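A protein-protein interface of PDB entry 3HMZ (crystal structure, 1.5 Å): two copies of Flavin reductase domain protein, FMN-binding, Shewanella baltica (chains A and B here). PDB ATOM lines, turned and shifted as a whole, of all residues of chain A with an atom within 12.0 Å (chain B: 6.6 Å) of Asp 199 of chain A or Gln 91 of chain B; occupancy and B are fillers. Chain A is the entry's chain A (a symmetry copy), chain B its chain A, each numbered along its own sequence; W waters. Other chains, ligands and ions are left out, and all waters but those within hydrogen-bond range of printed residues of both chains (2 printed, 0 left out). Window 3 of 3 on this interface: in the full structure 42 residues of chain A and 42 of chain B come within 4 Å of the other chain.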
ATOM      1  N   SER A 195     -10.587 -15.655  28.079  1.00  0.00           N
ATOM      2  CA  SER A 195     -11.485 -16.296  27.161  1.00  0.00           C
ATOM      3  C   SER A 195     -12.091 -15.270  26.206  1.00  0.00           C
ATOM      4  O   SER A 195     -12.495 -14.182  26.624  1.00  0.00           O
ATOM      5  CB  SER A 195     -12.625 -16.970  27.895  1.00  0.00           C
ATOM      6  OG  SER A 195     -13.347 -17.795  26.973  1.00  0.00           O
ATOM      7  N   PHE A 196     -12.172 -15.673  24.947  1.00  0.00           N
ATOM      8  CA  PHE A 196     -12.811 -14.947  23.848  1.00  0.00           C
ATOM      9  C   PHE A 196     -13.750 -15.870  23.084  1.00  0.00           C
ATOM     10  O   PHE A 196     -13.478 -17.064  22.966  1.00  0.00           O
ATOM     11  CB  PHE A 196     -11.776 -14.387  22.881  1.00  0.00           C
ATOM     12  CG  PHE A 196     -11.034 -13.218  23.451  1.00  0.00           C
ATOM     13  CD1 PHE A 196      -9.887 -13.367  24.177  1.00  0.00           C
ATOM     14  CD2 PHE A 196     -11.538 -11.965  23.298  1.00  0.00           C
ATOM     15  CE1 PHE A 196      -9.242 -12.277  24.701  1.00  0.00           C
ATOM     16  CE2 PHE A 196     -10.873 -10.886  23.820  1.00  0.00           C
ATOM     17  CZ  PHE A 196      -9.764 -11.044  24.544  1.00  0.00           C
ATOM     18  N   ASN A 197     -14.883 -15.322  22.614  1.00  0.00           N
ATOM     19  CA  ASN A 197     -15.877 -16.041  21.826  1.00  0.00           C
ATOM     20  C   ASN A 197     -16.104 -15.296  20.516  1.00  0.00           C
ATOM     21  O   ASN A 197     -16.455 -14.102  20.569  1.00  0.00           O
ATOM     22  CB  ASN A 197     -17.180 -16.091  22.609  1.00  0.00           C
ATOM     23  CG  ASN A 197     -17.083 -16.987  23.790  1.00  0.00           C
ATOM     24  OD1 ASN A 197     -17.125 -18.210  23.680  1.00  0.00           O
ATOM     25  ND2 ASN A 197     -17.005 -16.383  24.948  1.00  0.00           N
ATOM     26  N   ALA A 198     -15.910 -15.964  19.380  1.00  0.00           N
ATOM     27  CA  ALA A 198     -16.160 -15.391  18.076  1.00  0.00           C
ATOM     28  C   ALA A 198     -17.678 -15.212  17.908  1.00  0.00           C
ATOM     29  O   ALA A 198     -18.466 -15.903  18.570  1.00  0.00           O
ATOM     30  CB  ALA A 198     -15.548 -16.262  16.966  1.00  0.00           C
ATOM     31  N   ASP A 199     -18.043 -14.231  17.083  1.00  0.00           N
ATOM     32  CA  ASP A 199     -19.463 -13.900  16.814  1.00  0.00           C
ATOM     33  C   ASP A 199     -20.147 -15.016  16.056  1.00  0.00           C
ATOM     34  O   ASP A 199     -19.517 -15.763  15.288  1.00  0.00           O
ATOM     35  CB  ASP A 199     -19.612 -12.597  15.996  1.00  0.00           C
ATOM     36  CG  ASP A 199     -19.048 -11.369  16.701  1.00  0.00           C
ATOM     37  OD1 ASP A 199     -19.122 -11.268  17.946  1.00  0.00           O
ATOM     38  OD2 ASP A 199     -18.531 -10.474  15.986  1.00  0.00           O
ATOM     39  OXT ASP A 199     -21.371 -15.167  16.221  1.00  0.00           O
ATOM     40  N   THR B  86      -3.739 -12.829  15.832  1.00  0.00           N
ATOM     41  CA  THR B  86      -3.893 -12.063  17.052  1.00  0.00           C
ATOM     42  C   THR B  86      -5.339 -12.098  17.530  1.00  0.00           C
ATOM     43  O   THR B  86      -6.248 -12.444  16.779  1.00  0.00           O
ATOM     44  CB  THR B  86      -3.541 -10.605  16.810  1.00  0.00           C
ATOM     45  OG1 THR B  86      -4.519 -10.066  15.922  1.00  0.00           O
ATOM     46  CG2 THR B  86      -2.117 -10.448  16.297  1.00  0.00           C
ATOM     47  N   VAL B  87      -5.536 -11.668  18.773  1.00  0.00           N
ATOM     48  CA  VAL B  87      -6.889 -11.489  19.341  1.00  0.00           C
ATOM     49  C   VAL B  87      -7.730 -10.561  18.452  1.00  0.00           C
ATOM     50  O   VAL B  87      -8.914 -10.798  18.273  1.00  0.00           O
ATOM     51  CB  VAL B  87      -6.820 -10.998  20.790  1.00  0.00           C
ATOM     52  CG1 VAL B  87      -8.175 -10.398  21.239  1.00  0.00           C
ATOM     53  CG2 VAL B  87      -6.373 -12.133  21.690  1.00  0.00           C
ATOM     54  N   ALA B  88      -7.102  -9.532  17.855  1.00  0.00           N
ATOM     55  CA  ALA B  88      -7.792  -8.628  16.896  1.00  0.00           C
ATOM     56  C   ALA B  88      -8.376  -9.387  15.707  1.00  0.00           C
ATOM     57  O   ALA B  88      -9.362  -8.940  15.113  1.00  0.00           O
ATOM     58  CB  ALA B  88      -6.869  -7.538  16.395  1.00  0.00           C
ATOM     59  N   GLN B  89      -7.753 -10.525  15.366  1.00  0.00           N
ATOM     60  CA  GLN B  89      -8.161 -11.402  14.281  1.00  0.00           C
ATOM     61  C   GLN B  89      -9.025 -12.575  14.735  1.00  0.00           C
ATOM     62  O   GLN B  89      -9.153 -13.578  14.023  1.00  0.00           O
ATOM     63  CB  GLN B  89      -6.914 -11.907  13.563  1.00  0.00           C
ATOM     64  CG  GLN B  89      -6.115 -10.792  12.901  1.00  0.00           C
ATOM     65  CD  GLN B  89      -4.813 -11.316  12.337  1.00  0.00           C
ATOM     66  OE1 GLN B  89      -4.048 -11.949  13.040  1.00  0.00           O
ATOM     67  NE2 GLN B  89      -4.535 -11.002  11.070  1.00  0.00           N
ATOM     68  N   LEU B  90      -9.705 -12.415  15.885  1.00  0.00           N
ATOM     69  CA  LEU B  90     -10.589 -13.466  16.404  1.00  0.00           C
ATOM     70  C   LEU B  90     -11.659 -13.888  15.361  1.00  0.00           C
ATOM     71  O   LEU B  90     -11.790 -15.073  15.036  1.00  0.00           O
ATOM     72  CB  LEU B  90     -11.321 -12.976  17.663  1.00  0.00           C
ATOM     73  CG  LEU B  90     -12.404 -13.863  18.255  1.00  0.00           C
ATOM     74  CD1 LEU B  90     -11.827 -15.164  18.702  1.00  0.00           C
ATOM     75  CD2 LEU B  90     -13.040 -13.115  19.418  1.00  0.00           C
ATOM     76  N   GLN B  91     -12.367 -12.908  14.793  1.00  0.00           N
ATOM     77  CA  GLN B  91     -13.441 -13.232  13.833  1.00  0.00           C
ATOM     78  C   GLN B  91     -12.846 -13.818  12.560  1.00  0.00           C
ATOM     79  O   GLN B  91     -13.350 -14.813  12.047  1.00  0.00           O
ATOM     80  CB  GLN B  91     -14.321 -12.027  13.454  1.00  0.00           C
ATOM     81  CG  GLN B  91     -14.854 -11.159  14.560  1.00  0.00           C
ATOM     82  CD  GLN B  91     -15.439 -11.863  15.753  1.00  0.00           C
ATOM     83  OE1 GLN B  91     -16.109 -12.876  15.622  1.00  0.00           O
ATOM     84  NE2 GLN B  91     -15.275 -11.251  16.947  1.00  0.00           N
ATOM     85  N   LEU B  92     -11.762 -13.222  12.064  1.00  0.00           N
ATOM     86  CA  LEU B  92     -11.085 -13.710  10.868  1.00  0.00           C
ATOM     87  C   LEU B  92     -10.688 -15.174  11.024  1.00  0.00           C
ATOM     88  O   LEU B  92     -10.908 -16.009  10.130  1.00  0.00           O
ATOM     89  CB  LEU B  92      -9.846 -12.871  10.554  1.00  0.00           C
ATOM     90  CG  LEU B  92      -8.981 -13.172   9.321  1.00  0.00           C
ATOM     91  CD1 LEU B  92      -8.139 -11.938   8.882  1.00  0.00           C
ATOM     92  CD2 LEU B  92      -8.043 -14.351   9.534  1.00  0.00           C
ATOM     93  N   THR B  93     -10.125 -15.480  12.197  1.00  0.00           N
ATOM     94  CA  THR B  93      -9.615 -16.844  12.451  1.00  0.00           C
ATOM     95  C   THR B  93     -10.741 -17.863  12.456  1.00  0.00           C
ATOM     96  O   THR B  93     -10.670 -18.898  11.781  1.00  0.00           O
ATOM     97  CB  THR B  93      -8.804 -16.880  13.738  1.00  0.00           C
ATOM     98  OG1 THR B  93      -7.701 -15.965  13.624  1.00  0.00           O
ATOM     99  CG2 THR B  93      -8.283 -18.285  14.043  1.00  0.00           C
ATOM    100  N   HIS B  94     -11.810 -17.518  13.150  1.00  0.00           N
ATOM    101  CA  HIS B  94     -12.942 -18.419  13.195  1.00  0.00           C
ATOM    102  C   HIS B  94     -13.608 -18.568  11.828  1.00  0.00           C
ATOM    103  O   HIS B  94     -13.965 -19.672  11.429  1.00  0.00           O
ATOM    104  CB  HIS B  94     -13.935 -17.942  14.250  1.00  0.00           C
ATOM    105  CG  HIS B  94     -14.981 -18.962  14.554  1.00  0.00           C
ATOM    106  ND1 HIS B  94     -16.234 -18.849  14.029  1.00  0.00           N
ATOM    107  CD2 HIS B  94     -14.931 -20.163  15.184  1.00  0.00           C
ATOM    108  CE1 HIS B  94     -16.962 -19.892  14.407  1.00  0.00           C
ATOM    109  NE2 HIS B  94     -16.198 -20.703  15.120  1.00  0.00           N
ATOM    110  N   ARG B  95     -13.694 -17.460  11.087  1.00  0.00           N
ATOM    111  CA  ARG B  95     -14.337 -17.466   9.769  1.00  0.00           C
ATOM    112  C   ARG B  95     -13.585 -18.304   8.759  1.00  0.00           C
ATOM    113  O   ARG B  95     -14.198 -19.102   8.035  1.00  0.00           O
ATOM    114  CB  ARG B  95     -14.522 -16.047   9.226  1.00  0.00           C
ATOM    115  CG  ARG B  95     -15.599 -15.254   9.929  1.00  0.00           C
ATOM    116  CD  ARG B  95     -15.713 -13.866   9.297  1.00  0.00           C
ATOM    117  NE  ARG B  95     -16.613 -13.020  10.059  1.00  0.00           N
ATOM    118  CZ  ARG B  95     -17.084 -11.856   9.637  1.00  0.00           C
ATOM    119  NH1 ARG B  95     -16.771 -11.407   8.439  1.00  0.00           N
ATOM    120  NH2 ARG B  95     -17.891 -11.152  10.414  1.00  0.00           N
ATOM    121  N   VAL B  96     -12.260 -18.138   8.686  1.00  0.00           N
ATOM    122  CA  VAL B  96     -11.476 -18.938   7.719  1.00  0.00           C
ATOM    123  C   VAL B  96     -11.453 -20.421   8.077  1.00  0.00           C
ATOM    124  O   VAL B  96     -11.179 -21.243   7.210  1.00  0.00           O
ATOM    125  CB  VAL B  96     -10.036 -18.436   7.478  1.00  0.00           C
ATOM    126  CG1 VAL B  96     -10.065 -16.973   6.915  1.00  0.00           C
ATOM    127  CG2 VAL B  96      -9.183 -18.523   8.730  1.00  0.00           C
ATOM    128  N   CYS B 111     -14.103 -13.224   4.512  1.00  0.00           N
ATOM    129  CA  CYS B 111     -13.523 -13.448   5.824  1.00  0.00           C
ATOM    130  C   CYS B 111     -12.687 -12.243   6.299  1.00  0.00           C
ATOM    131  O   CYS B 111     -12.213 -12.254   7.426  1.00  0.00           O
ATOM    132  CB  CYS B 111     -12.661 -14.720   5.818  1.00  0.00           C
ATOM    133  SG  CYS B 111     -13.582 -16.266   5.650  1.00  0.00           S
ATOM    134  N   LEU B 181      -4.034 -16.528  19.938  1.00  0.00           N
ATOM    135  CA  LEU B 181      -5.252 -17.244  20.175  1.00  0.00           C
ATOM    136  C   LEU B 181      -4.993 -18.733  20.235  1.00  0.00           C
ATOM    137  O   LEU B 181      -4.220 -19.264  19.459  1.00  0.00           O
ATOM    138  CB  LEU B 181      -6.246 -16.976  19.056  1.00  0.00           C
ATOM    139  CG  LEU B 181      -6.863 -15.584  18.971  1.00  0.00           C
ATOM    140  CD1 LEU B 181      -7.595 -15.393  17.595  1.00  0.00           C
ATOM    141  CD2 LEU B 181      -7.826 -15.363  20.144  1.00  0.00           C
ATOM    142  N   GLY B 187     -16.881 -21.418  19.032  1.00  0.00           N
ATOM    143  CA  GLY B 187     -16.257 -20.125  18.744  1.00  0.00           C
ATOM    144  C   GLY B 187     -15.326 -19.678  19.856  1.00  0.00           C
ATOM    145  O   GLY B 187     -14.885 -18.532  19.846  1.00  0.00           O
HETATM  146  O   HOH W   1     -16.697 -11.765  19.190  1.00  0.00           O
HETATM  147  O   HOH W   2     -17.308 -16.782  12.908  1.00  0.00           O
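OE1 of Gln 91 of chain B lies within hydrogen-bond range of N of Asp 199 of chain A (2.8 Å).
The backbone carbonyl oxygen (O) of Gly 187 of chain B sits at hydrogen-bond distance from the backbone NH (N) of Ala 198 of chain A, 2.8 Å away.
Among the printed residues, pairs that only touch across the chains: Phe 196 of chain A with Val 87 of chain B (3.7 Å), Phe 196 of chain A with Leu 90 of chain B (3.9 Å), Phe 196 of chain A with Gly 187 of chain B (3.7 Å), Asn 197 of chain A with Leu 90 of chain B (3.7 Å), Asn 197 of chain A with Gly 187 of chain B (3.3 Å), Ala 198 of chain A with Gln 91 of chain B (3.5 Å) and Ala 198 of chain A with His 94 of chain B (3.6 Å).
Of the printed residues of chain B, Asp 199 of chain A touches Gln 91 (2.8 Å).
Of the printed residues of chain A, Gln 91 of chain B touches Ala 198 and Asp 199.
No residue of chain A comes within 4 Å of Leu 92 of chain B.
His 94 of chain B touches just one residue of chain A: Ala 198 (3.6 Å).
No residue of chain A comes within 4 Å of Cys 111 of chain B.
Of the printed residues of chain B, Phe 196 of chain A touches Val 87 (3.7 Å), Leu 90 (3.9 Å) and Gly 187 (3.7 Å).
Printed residues of chain A within 4 Å of Gly 187 of chain B: Phe 196, Asn 197 and Ala 198.
Of the printed residues of chain A, Val 87 of chain B touches Phe 196.
Printed residues of chain A within 4 Å of Leu 90 of chain B: Phe 196 (3.9 Å) and Asn 197 (3.7 Å).
Of the printed residues of chain B, Asn 197 of chain A touches Leu 90 (3.7 Å) and Gly 187 (3.3 Å).
Ser 195 of chain A touches none of the printed residues of chain B.
Leu 181 of chain B touches none of the printed residues of chain A.
The nearest printed residue of chain B that does not touch Asp 199 of chain A is His 94 of chain B (4.7 Å).
The nearest printed residue of chain A that does not touch Gln 91 of chain B is Asn 197 of chain A (4.8 Å).
Hydrophobic or aromatic side chains of chain B that line the printed part of chain A: Val 87, Leu 90 and His 94.
No position is printed for both chains.
Of the 9 pairs that touch across the chains among the printed residues, none has its exchanged pair printed and touching as well.
Water W2 lies within hydrogen-bond range of a ring nitrogen (ND1) of His 94 of chain B (2.6 Å) and the chain-end carboxylate of Asp 199 of chain A (3.4 Å).
Water W1 lies within hydrogen-bond range of the side-chain amide nitrogen of Gln 91 of chain B (2.7 Å), the backbone carbonyl oxygen of Asn 197 of chain A (2.7 Å) and the side-chain carboxylate of Asp 199 of chain A (2.8 Å).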
